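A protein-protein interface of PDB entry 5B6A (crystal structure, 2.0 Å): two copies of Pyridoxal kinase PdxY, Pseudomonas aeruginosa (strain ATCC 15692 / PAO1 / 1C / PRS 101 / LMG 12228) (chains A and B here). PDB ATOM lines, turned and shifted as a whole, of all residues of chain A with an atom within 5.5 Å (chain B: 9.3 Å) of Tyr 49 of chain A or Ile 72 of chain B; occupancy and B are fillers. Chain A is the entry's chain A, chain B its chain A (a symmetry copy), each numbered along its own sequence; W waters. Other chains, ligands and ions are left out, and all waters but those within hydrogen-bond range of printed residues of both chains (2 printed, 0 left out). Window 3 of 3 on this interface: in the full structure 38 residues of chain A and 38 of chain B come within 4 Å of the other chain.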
ATOM      1  N   PHE A  16      17.301  19.346 -21.524  1.00  0.00           N
ATOM      2  CA  PHE A  16      16.467  19.090 -20.370  1.00  0.00           C
ATOM      3  C   PHE A  16      17.326  19.256 -19.116  1.00  0.00           C
ATOM      4  O   PHE A  16      18.473  18.805 -19.089  1.00  0.00           O
ATOM      5  CB  PHE A  16      15.927  17.657 -20.425  1.00  0.00           C
ATOM      6  CG  PHE A  16      15.162  17.263 -19.194  1.00  0.00           C
ATOM      7  CD1 PHE A  16      15.820  16.690 -18.090  1.00  0.00           C
ATOM      8  CD2 PHE A  16      13.802  17.514 -19.105  1.00  0.00           C
ATOM      9  CE1 PHE A  16      15.118  16.362 -16.937  1.00  0.00           C
ATOM     10  CE2 PHE A  16      13.099  17.184 -17.947  1.00  0.00           C
ATOM     11  CZ  PHE A  16      13.762  16.617 -16.871  1.00  0.00           C
ATOM     12  N   ASN A  45      20.752  16.092 -21.765  1.00  0.00           N
ATOM     13  CA  ASN A  45      20.608  16.078 -20.297  1.00  0.00           C
ATOM     14  C   ASN A  45      22.017  15.949 -19.695  1.00  0.00           C
ATOM     15  O   ASN A  45      22.981  15.705 -20.445  1.00  0.00           O
ATOM     16  CB  ASN A  45      19.654  14.950 -19.816  1.00  0.00           C
ATOM     17  CG  ASN A  45      20.147  13.561 -20.205  1.00  0.00           C
ATOM     18  OD1 ASN A  45      21.042  12.982 -19.539  1.00  0.00           O
ATOM     19  ND2 ASN A  45      19.626  13.038 -21.289  1.00  0.00           N
ATOM     20  N   HIS A  46      22.171  16.172 -18.386  1.00  0.00           N
ATOM     21  CA  HIS A  46      23.515  16.151 -17.789  1.00  0.00           C
ATOM     22  C   HIS A  46      24.054  14.719 -17.683  1.00  0.00           C
ATOM     23  O   HIS A  46      23.285  13.738 -17.769  1.00  0.00           O
ATOM     24  CB  HIS A  46      23.583  16.938 -16.456  1.00  0.00           C
ATOM     25  CG  HIS A  46      22.807  16.324 -15.323  1.00  0.00           C
ATOM     26  ND1 HIS A  46      23.085  15.068 -14.814  1.00  0.00           N
ATOM     27  CD2 HIS A  46      21.783  16.809 -14.578  1.00  0.00           C
ATOM     28  CE1 HIS A  46      22.251  14.795 -13.824  1.00  0.00           C
ATOM     29  NE2 HIS A  46      21.456  15.839 -13.656  1.00  0.00           N
ATOM     30  N   THR A  47      25.362  14.589 -17.495  1.00  0.00           N
ATOM     31  CA  THR A  47      25.990  13.259 -17.563  1.00  0.00           C
ATOM     32  C   THR A  47      25.731  12.343 -16.366  1.00  0.00           C
ATOM     33  O   THR A  47      25.931  11.130 -16.484  1.00  0.00           O
ATOM     34  CB  THR A  47      27.526  13.323 -17.797  1.00  0.00           C
ATOM     35  OG1 THR A  47      28.135  14.006 -16.706  1.00  0.00           O
ATOM     36  CG2 THR A  47      27.869  14.030 -19.114  1.00  0.00           C
ATOM     37  N   GLN A  48      25.287  12.907 -15.241  1.00  0.00           N
ATOM     38  CA  GLN A  48      25.088  12.113 -14.019  1.00  0.00           C
ATOM     39  C   GLN A  48      23.919  11.141 -14.085  1.00  0.00           C
ATOM     40  O   GLN A  48      23.827  10.260 -13.239  1.00  0.00           O
ATOM     41  CB  GLN A  48      25.039  12.984 -12.764  1.00  0.00           C
ATOM     42  CG  GLN A  48      26.311  13.806 -12.555  1.00  0.00           C
ATOM     43  CD  GLN A  48      27.572  13.007 -12.827  1.00  0.00           C
ATOM     44  OE1 GLN A  48      28.376  13.359 -13.696  1.00  0.00           O
ATOM     45  NE2 GLN A  48      27.749  11.921 -12.089  1.00  0.00           N
ATOM     46  N   TYR A  49      23.065  11.274 -15.108  1.00  0.00           N
ATOM     47  CA  TYR A  49      22.043  10.240 -15.432  1.00  0.00           C
ATOM     48  C   TYR A  49      22.686   8.926 -15.920  1.00  0.00           C
ATOM     49  O   TYR A  49      22.037   7.882 -15.896  1.00  0.00           O
ATOM     50  CB  TYR A  49      21.063  10.725 -16.500  1.00  0.00           C
ATOM     51  CG  TYR A  49      20.059  11.770 -16.021  1.00  0.00           C
ATOM     52  CD1 TYR A  49      18.838  11.395 -15.438  1.00  0.00           C
ATOM     53  CD2 TYR A  49      20.337  13.121 -16.147  1.00  0.00           C
ATOM     54  CE1 TYR A  49      17.917  12.356 -15.005  1.00  0.00           C
ATOM     55  CE2 TYR A  49      19.441  14.090 -15.711  1.00  0.00           C
ATOM     56  CZ  TYR A  49      18.231  13.709 -15.140  1.00  0.00           C
ATOM     57  OH  TYR A  49      17.358  14.696 -14.717  1.00  0.00           O
ATOM     58  N   GLY A  50      23.946   8.989 -16.373  1.00  0.00           N
ATOM     59  CA  GLY A  50      24.672   7.800 -16.871  1.00  0.00           C
ATOM     60  C   GLY A  50      24.311   7.481 -18.317  1.00  0.00           C
ATOM     61  O   GLY A  50      24.677   6.427 -18.846  1.00  0.00           O
ATOM     62  N   ARG A  51      23.555   8.389 -18.932  1.00  0.00           N
ATOM     63  CA  ARG A  51      23.146   8.321 -20.334  1.00  0.00           C
ATOM     64  C   ARG A  51      22.823   9.748 -20.798  1.00  0.00           C
ATOM     65  O   ARG A  51      22.297  10.541 -20.023  1.00  0.00           O
ATOM     66  CB  ARG A  51      21.920   7.422 -20.480  1.00  0.00           C
ATOM     67  CG  ARG A  51      20.722   7.871 -19.636  1.00  0.00           C
ATOM     68  CD  ARG A  51      19.644   6.834 -19.495  1.00  0.00           C
ATOM     69  NE  ARG A  51      19.324   6.270 -20.794  1.00  0.00           N
ATOM     70  CZ  ARG A  51      19.529   4.997 -21.127  1.00  0.00           C
ATOM     71  NH1 ARG A  51      20.017   4.148 -20.245  1.00  0.00           N
ATOM     72  NH2 ARG A  51      19.216   4.573 -22.347  1.00  0.00           N
ATOM     73  N   ARG A 218      19.295  11.669  -4.376  1.00  0.00           N
ATOM     74  CA  ARG A 218      20.305  11.853  -5.418  1.00  0.00           C
ATOM     75  C   ARG A 218      20.805  13.304  -5.413  1.00  0.00           C
ATOM     76  O   ARG A 218      19.999  14.225  -5.500  1.00  0.00           O
ATOM     77  CB  ARG A 218      19.705  11.515  -6.782  1.00  0.00           C
ATOM     78  CG  ARG A 218      19.938  10.091  -7.264  1.00  0.00           C
ATOM     79  CD  ARG A 218      19.893  10.015  -8.789  1.00  0.00           C
ATOM     80  NE  ARG A 218      18.554  10.297  -9.333  1.00  0.00           N
ATOM     81  CZ  ARG A 218      18.182  10.141 -10.609  1.00  0.00           C
ATOM     82  NH1 ARG A 218      19.037   9.702 -11.532  1.00  0.00           N
ATOM     83  NH2 ARG A 218      16.937  10.428 -10.964  1.00  0.00           N
ATOM     84  N   TYR A 265      15.030  15.746  -8.756  1.00  0.00           N
ATOM     85  CA  TYR A 265      16.451  15.551  -8.980  1.00  0.00           C
ATOM     86  C   TYR A 265      17.046  16.807  -9.631  1.00  0.00           C
ATOM     87  O   TYR A 265      18.142  17.255  -9.265  1.00  0.00           O
ATOM     88  CB  TYR A 265      16.654  14.304  -9.857  1.00  0.00           C
ATOM     89  CG  TYR A 265      18.093  13.966 -10.210  1.00  0.00           C
ATOM     90  CD1 TYR A 265      19.127  14.095  -9.257  1.00  0.00           C
ATOM     91  CD2 TYR A 265      18.424  13.479 -11.490  1.00  0.00           C
ATOM     92  CE1 TYR A 265      20.437  13.784  -9.584  1.00  0.00           C
ATOM     93  CE2 TYR A 265      19.741  13.146 -11.816  1.00  0.00           C
ATOM     94  CZ  TYR A 265      20.733  13.309 -10.855  1.00  0.00           C
ATOM     95  OH  TYR A 265      22.023  12.988 -11.144  1.00  0.00           O
ATOM     96  N   GLU A 266      16.327  17.380 -10.591  1.00  0.00           N
ATOM     97  CA  GLU A 266      16.763  18.626 -11.244  1.00  0.00           C
ATOM     98  C   GLU A 266      16.426  19.841 -10.388  1.00  0.00           C
ATOM     99  O   GLU A 266      15.372  19.875  -9.742  1.00  0.00           O
ATOM    100  CB  GLU A 266      16.113  18.766 -12.618  1.00  0.00           C
ATOM    101  CG  GLU A 266      16.561  17.697 -13.604  1.00  0.00           C
ATOM    102  CD  GLU A 266      17.972  17.909 -14.181  1.00  0.00           C
ATOM    103  OE1 GLU A 266      18.610  18.978 -13.951  1.00  0.00           O
ATOM    104  OE2 GLU A 266      18.428  17.012 -14.921  1.00  0.00           O
ATOM    105  N   TRP B  36      12.798  23.933 -22.033  1.00  0.00           N
ATOM    106  CA  TRP B  36      13.874  23.052 -22.523  1.00  0.00           C
ATOM    107  C   TRP B  36      14.409  23.657 -23.823  1.00  0.00           C
ATOM    108  O   TRP B  36      13.748  23.551 -24.852  1.00  0.00           O
ATOM    109  CB  TRP B  36      13.362  21.629 -22.786  1.00  0.00           C
ATOM    110  CG  TRP B  36      12.567  20.967 -21.657  1.00  0.00           C
ATOM    111  CD1 TRP B  36      12.387  21.424 -20.378  1.00  0.00           C
ATOM    112  CD2 TRP B  36      11.875  19.712 -21.733  1.00  0.00           C
ATOM    113  NE1 TRP B  36      11.609  20.548 -19.665  1.00  0.00           N
ATOM    114  CE2 TRP B  36      11.287  19.481 -20.464  1.00  0.00           C
ATOM    115  CE3 TRP B  36      11.698  18.758 -22.751  1.00  0.00           C
ATOM    116  CZ2 TRP B  36      10.539  18.335 -20.180  1.00  0.00           C
ATOM    117  CZ3 TRP B  36      10.942  17.601 -22.467  1.00  0.00           C
ATOM    118  CH2 TRP B  36      10.371  17.410 -21.192  1.00  0.00           C
ATOM    119  N   LEU B  65      18.768  14.633 -29.877  1.00  0.00           N
ATOM    120  CA  LEU B  65      18.625  15.286 -28.557  1.00  0.00           C
ATOM    121  C   LEU B  65      17.329  14.870 -27.836  1.00  0.00           C
ATOM    122  O   LEU B  65      17.355  14.503 -26.648  1.00  0.00           O
ATOM    123  CB  LEU B  65      18.762  16.817 -28.680  1.00  0.00           C
ATOM    124  CG  LEU B  65      20.206  17.318 -28.950  1.00  0.00           C
ATOM    125  CD1 LEU B  65      20.207  18.770 -29.392  1.00  0.00           C
ATOM    126  CD2 LEU B  65      21.143  17.122 -27.760  1.00  0.00           C
ATOM    127  N   VAL B  66      16.222  14.832 -28.578  1.00  0.00           N
ATOM    128  CA  VAL B  66      14.933  14.445 -28.012  1.00  0.00           C
ATOM    129  C   VAL B  66      14.951  12.963 -27.623  1.00  0.00           C
ATOM    130  O   VAL B  66      14.401  12.566 -26.579  1.00  0.00           O
ATOM    131  CB  VAL B  66      13.784  14.841 -28.978  1.00  0.00           C
ATOM    132  CG1 VAL B  66      12.452  14.158 -28.628  1.00  0.00           C
ATOM    133  CG2 VAL B  66      13.638  16.356 -28.958  1.00  0.00           C
ATOM    134  N   ASP B  67      15.627  12.158 -28.441  1.00  0.00           N
ATOM    135  CA  ASP B  67      15.863  10.754 -28.111  1.00  0.00           C
ATOM    136  C   ASP B  67      16.581  10.592 -26.768  1.00  0.00           C
ATOM    137  O   ASP B  67      16.265   9.673 -26.014  1.00  0.00           O
ATOM    138  CB  ASP B  67      16.644  10.045 -29.230  1.00  0.00           C
ATOM    139  CG  ASP B  67      16.647   8.557 -29.058  1.00  0.00           C
ATOM    140  OD1 ASP B  67      15.568   7.964 -29.205  1.00  0.00           O
ATOM    141  OD2 ASP B  67      17.710   7.992 -28.717  1.00  0.00           O
ATOM    142  N   GLY B  68      17.541  11.478 -26.482  1.00  0.00           N
ATOM    143  CA  GLY B  68      18.243  11.475 -25.197  1.00  0.00           C
ATOM    144  C   GLY B  68      17.287  11.718 -24.037  1.00  0.00           C
ATOM    145  O   GLY B  68      17.366  11.032 -23.022  1.00  0.00           O
ATOM    146  N   ILE B  69      16.370  12.684 -24.206  1.00  0.00           N
ATOM    147  CA  ILE B  69      15.379  13.031 -23.165  1.00  0.00           C
ATOM    148  C   ILE B  69      14.414  11.857 -22.958  1.00  0.00           C
ATOM    149  O   ILE B  69      14.086  11.532 -21.824  1.00  0.00           O
ATOM    150  CB  ILE B  69      14.616  14.344 -23.496  1.00  0.00           C
ATOM    151  CG1 ILE B  69      15.616  15.508 -23.713  1.00  0.00           C
ATOM    152  CG2 ILE B  69      13.565  14.668 -22.421  1.00  0.00           C
ATOM    153  CD1 ILE B  69      15.002  16.777 -24.296  1.00  0.00           C
ATOM    154  N   ALA B  70      13.958  11.238 -24.050  1.00  0.00           N
ATOM    155  CA  ALA B  70      13.180   9.984 -23.978  1.00  0.00           C
ATOM    156  C   ALA B  70      13.937   8.901 -23.184  1.00  0.00           C
ATOM    157  O   ALA B  70      13.328   8.169 -22.376  1.00  0.00           O
ATOM    158  CB  ALA B  70      12.838   9.487 -25.366  1.00  0.00           C
ATOM    159  N   GLY B  71      15.262   8.845 -23.370  1.00  0.00           N
ATOM    160  CA  GLY B  71      16.102   7.841 -22.718  1.00  0.00           C
ATOM    161  C   GLY B  71      16.149   7.967 -21.205  1.00  0.00           C
ATOM    162  O   GLY B  71      16.345   6.976 -20.504  1.00  0.00           O
ATOM    163  N   ILE B  72      15.972   9.177 -20.685  1.00  0.00           N
ATOM    164  CA  ILE B  72      15.836   9.315 -19.230  1.00  0.00           C
ATOM    165  C   ILE B  72      14.376   9.308 -18.716  1.00  0.00           C
ATOM    166  O   ILE B  72      14.151   9.522 -17.516  1.00  0.00           O
ATOM    167  CB  ILE B  72      16.642  10.518 -18.667  1.00  0.00           C
ATOM    168  CG1 ILE B  72      16.251  11.818 -19.393  1.00  0.00           C
ATOM    169  CG2 ILE B  72      18.131  10.222 -18.761  1.00  0.00           C
ATOM    170  CD1 ILE B  72      16.677  13.094 -18.698  1.00  0.00           C
ATOM    171  N   GLY B  73      13.420   9.064 -19.620  1.00  0.00           N
ATOM    172  CA  GLY B  73      12.006   8.894 -19.272  1.00  0.00           C
ATOM    173  C   GLY B  73      11.239  10.177 -18.978  1.00  0.00           C
ATOM    174  O   GLY B  73      10.261  10.152 -18.232  1.00  0.00           O
ATOM    175  N   GLU B  74      11.666  11.289 -19.581  1.00  0.00           N
ATOM    176  CA  GLU B  74      11.134  12.621 -19.244  1.00  0.00           C
ATOM    177  C   GLU B  74      10.233  13.257 -20.303  1.00  0.00           C
ATOM    178  O   GLU B  74       9.652  14.332 -20.074  1.00  0.00           O
ATOM    179  CB  GLU B  74      12.285  13.581 -18.910  1.00  0.00           C
ATOM    180  CG  GLU B  74      13.053  13.226 -17.638  1.00  0.00           C
ATOM    181  CD  GLU B  74      12.304  13.558 -16.356  1.00  0.00           C
ATOM    182  OE1 GLU B  74      11.208  14.180 -16.400  1.00  0.00           O
ATOM    183  OE2 GLU B  74      12.822  13.204 -15.287  1.00  0.00           O
ATOM    184  N   LEU B  75      10.118  12.596 -21.450  1.00  0.00           N
ATOM    185  CA  LEU B  75       9.422  13.165 -22.596  1.00  0.00           C
ATOM    186  C   LEU B  75       7.928  13.416 -22.337  1.00  0.00           C
ATOM    187  O   LEU B  75       7.371  14.392 -22.841  1.00  0.00           O
ATOM    188  CB  LEU B  75       9.634  12.285 -23.835  1.00  0.00           C
ATOM    189  CG  LEU B  75       9.793  12.998 -25.170  1.00  0.00           C
ATOM    190  CD1 LEU B  75      10.833  14.121 -25.119  1.00  0.00           C
ATOM    191  CD2 LEU B  75      10.126  11.984 -26.257  1.00  0.00           C
ATOM    192  N   GLY B  76       7.309  12.560 -21.517  1.00  0.00           N
ATOM    193  CA  GLY B  76       5.908  12.692 -21.108  1.00  0.00           C
ATOM    194  C   GLY B  76       5.606  13.951 -20.314  1.00  0.00           C
ATOM    195  O   GLY B  76       4.457  14.367 -20.239  1.00  0.00           O
ATOM    196  N   ASN B  77       6.635  14.564 -19.724  1.00  0.00           N
ATOM    197  CA  ASN B  77       6.472  15.807 -18.953  1.00  0.00           C
ATOM    198  C   ASN B  77       6.408  17.077 -19.799  1.00  0.00           C
ATOM    199  O   ASN B  77       6.088  18.154 -19.290  1.00  0.00           O
ATOM    200  CB  ASN B  77       7.551  15.903 -17.873  1.00  0.00           C
ATOM    201  CG  ASN B  77       7.386  14.831 -16.816  1.00  0.00           C
ATOM    202  OD1 ASN B  77       6.264  14.479 -16.443  1.00  0.00           O
ATOM    203  ND2 ASN B  77       8.490  14.278 -16.356  1.00  0.00           N
ATOM    204  N   ARG B 101       6.511  12.511 -31.788  1.00  0.00           N
ATOM    205  CA  ARG B 101       7.038  11.691 -30.704  1.00  0.00           C
ATOM    206  C   ARG B 101       6.554  12.198 -29.329  1.00  0.00           C
ATOM    207  O   ARG B 101       6.163  11.415 -28.465  1.00  0.00           O
ATOM    208  CB  ARG B 101       8.576  11.649 -30.744  1.00  0.00           C
ATOM    209  CG  ARG B 101       9.127  10.423 -30.041  1.00  0.00           C
ATOM    210  CD  ARG B 101      10.624  10.557 -29.778  1.00  0.00           C
ATOM    211  NE  ARG B 101      11.051   9.390 -29.022  1.00  0.00           N
ATOM    212  CZ  ARG B 101      12.254   8.824 -29.081  1.00  0.00           C
ATOM    213  NH1 ARG B 101      13.228   9.312 -29.853  1.00  0.00           N
ATOM    214  NH2 ARG B 101      12.468   7.747 -28.358  1.00  0.00           N
HETATM  215  O   HOH W   1      14.940  14.050 -13.742  1.00  0.00           O
HETATM  216  O   HOH W   2      19.773  10.275 -22.068  1.00  0.00           O
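The backbone carbonyl oxygen (O) of Gly 71 of chain B is in hydrogen-bond range of the guanidinium group (NE) of Arg 51 of chain A (3.1 Å). The side-chain amide nitrogen (ND2) of Asn 45 of chain A lies within hydrogen-bond range of the backbone carbonyl oxygen (O) of Gly 68 of chain B.
The backbone carbonyl oxygen (O) of Ile 69 of chain B lies within hydrogen-bond range of the backbone NH (N) of Glu 74 of chain B (3.3 Å). OH of Tyr 49 of chain A sits at hydrogen-bond distance from OE2 of Glu 266 of chain A (2.6 Å). OD1 of Asn 45 of chain A lies close to O of Arg 51 of chain A, 2.8 Å away. The side-chain carboxylate (OE1) of Glu 74 of chain B lies within hydrogen-bond range of the side-chain amide nitrogen (ND2) of Asn 77 of chain B (2.7 Å).
Among the printed residues, pairs that only touch across the chains: Phe 16 of chain A with Glu 74 of chain B (3.4 Å), Phe 16 of chain A with Trp 36 of chain B (3.5 Å), Tyr 49 of chain A with Ile 72 of chain B (3.6 Å), Arg 51 of chain A with Ile 72 of chain B (3.6 Å), Asn 45 of chain A with Ile 72 of chain B (3.7 Å), Phe 16 of chain A with Ile 72 of chain B (3.7 Å) and Phe 16 of chain A with Ile 69 of chain B (3.9 Å).
Tyr 49 of chain A touches just one residue of chain B: Ile 72 (3.6 Å). Of the printed residues of chain A, Ile 72 of chain B touches Phe 16 (3.7 Å), Asn 45 (3.7 Å), Tyr 49 (3.6 Å) and Arg 51 (3.6 Å). Gly 50 of chain A touches none of the printed residues of chain B. Of the printed residues of chain A, Trp 36 of chain B touches Phe 16. Of the printed residues of chain A, Gly 68 of chain B touches Asn 45. Of the printed residues of chain B, Phe 16 of chain A touches Trp 36, Ile 69, Ile 72 and Glu 74. Of the printed residues of chain A, Glu 74 of chain B touches Phe 16 (3.4 Å). Leu 65 of chain B touches none of the printed residues of chain A. Arg 101 of chain B touches none of the printed residues of chain A. The nearest printed residue of chain B that does not touch Asn 45 of chain A is Ile 69 of chain B (4.4 Å).
Printed residues of chain B that touch a printed residue of chain A: Trp 36, Gly 68, Ile 69, Gly 71, Ile 72 and Glu 74. Of the 11 printed residues of chain A, 4 touch a printed residue of chain B. Hydrophobic or aromatic side chains of chain A within 4 Å of the printed part of chain B: Phe 16 and Tyr 49. Among the printed residues, no Asp or Glu carboxylate lies within 4 Å of a Lys or Arg side-chain nitrogen of the other chain.
No position is printed for both chains.
Water W1 bridges the side-chain hydroxyl of Tyr 49 of chain A (2.7 Å) and the side-chain carboxylate of Glu 74 of chain B (2.8 Å). Water W2 lies within hydrogen-bond range of the backbone carbonyl oxygen of Gly 68 of chain B, the side-chain amide nitrogen of Asn 45 of chain A and the backbone carbonyl oxygen of Arg 51 of chain A.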
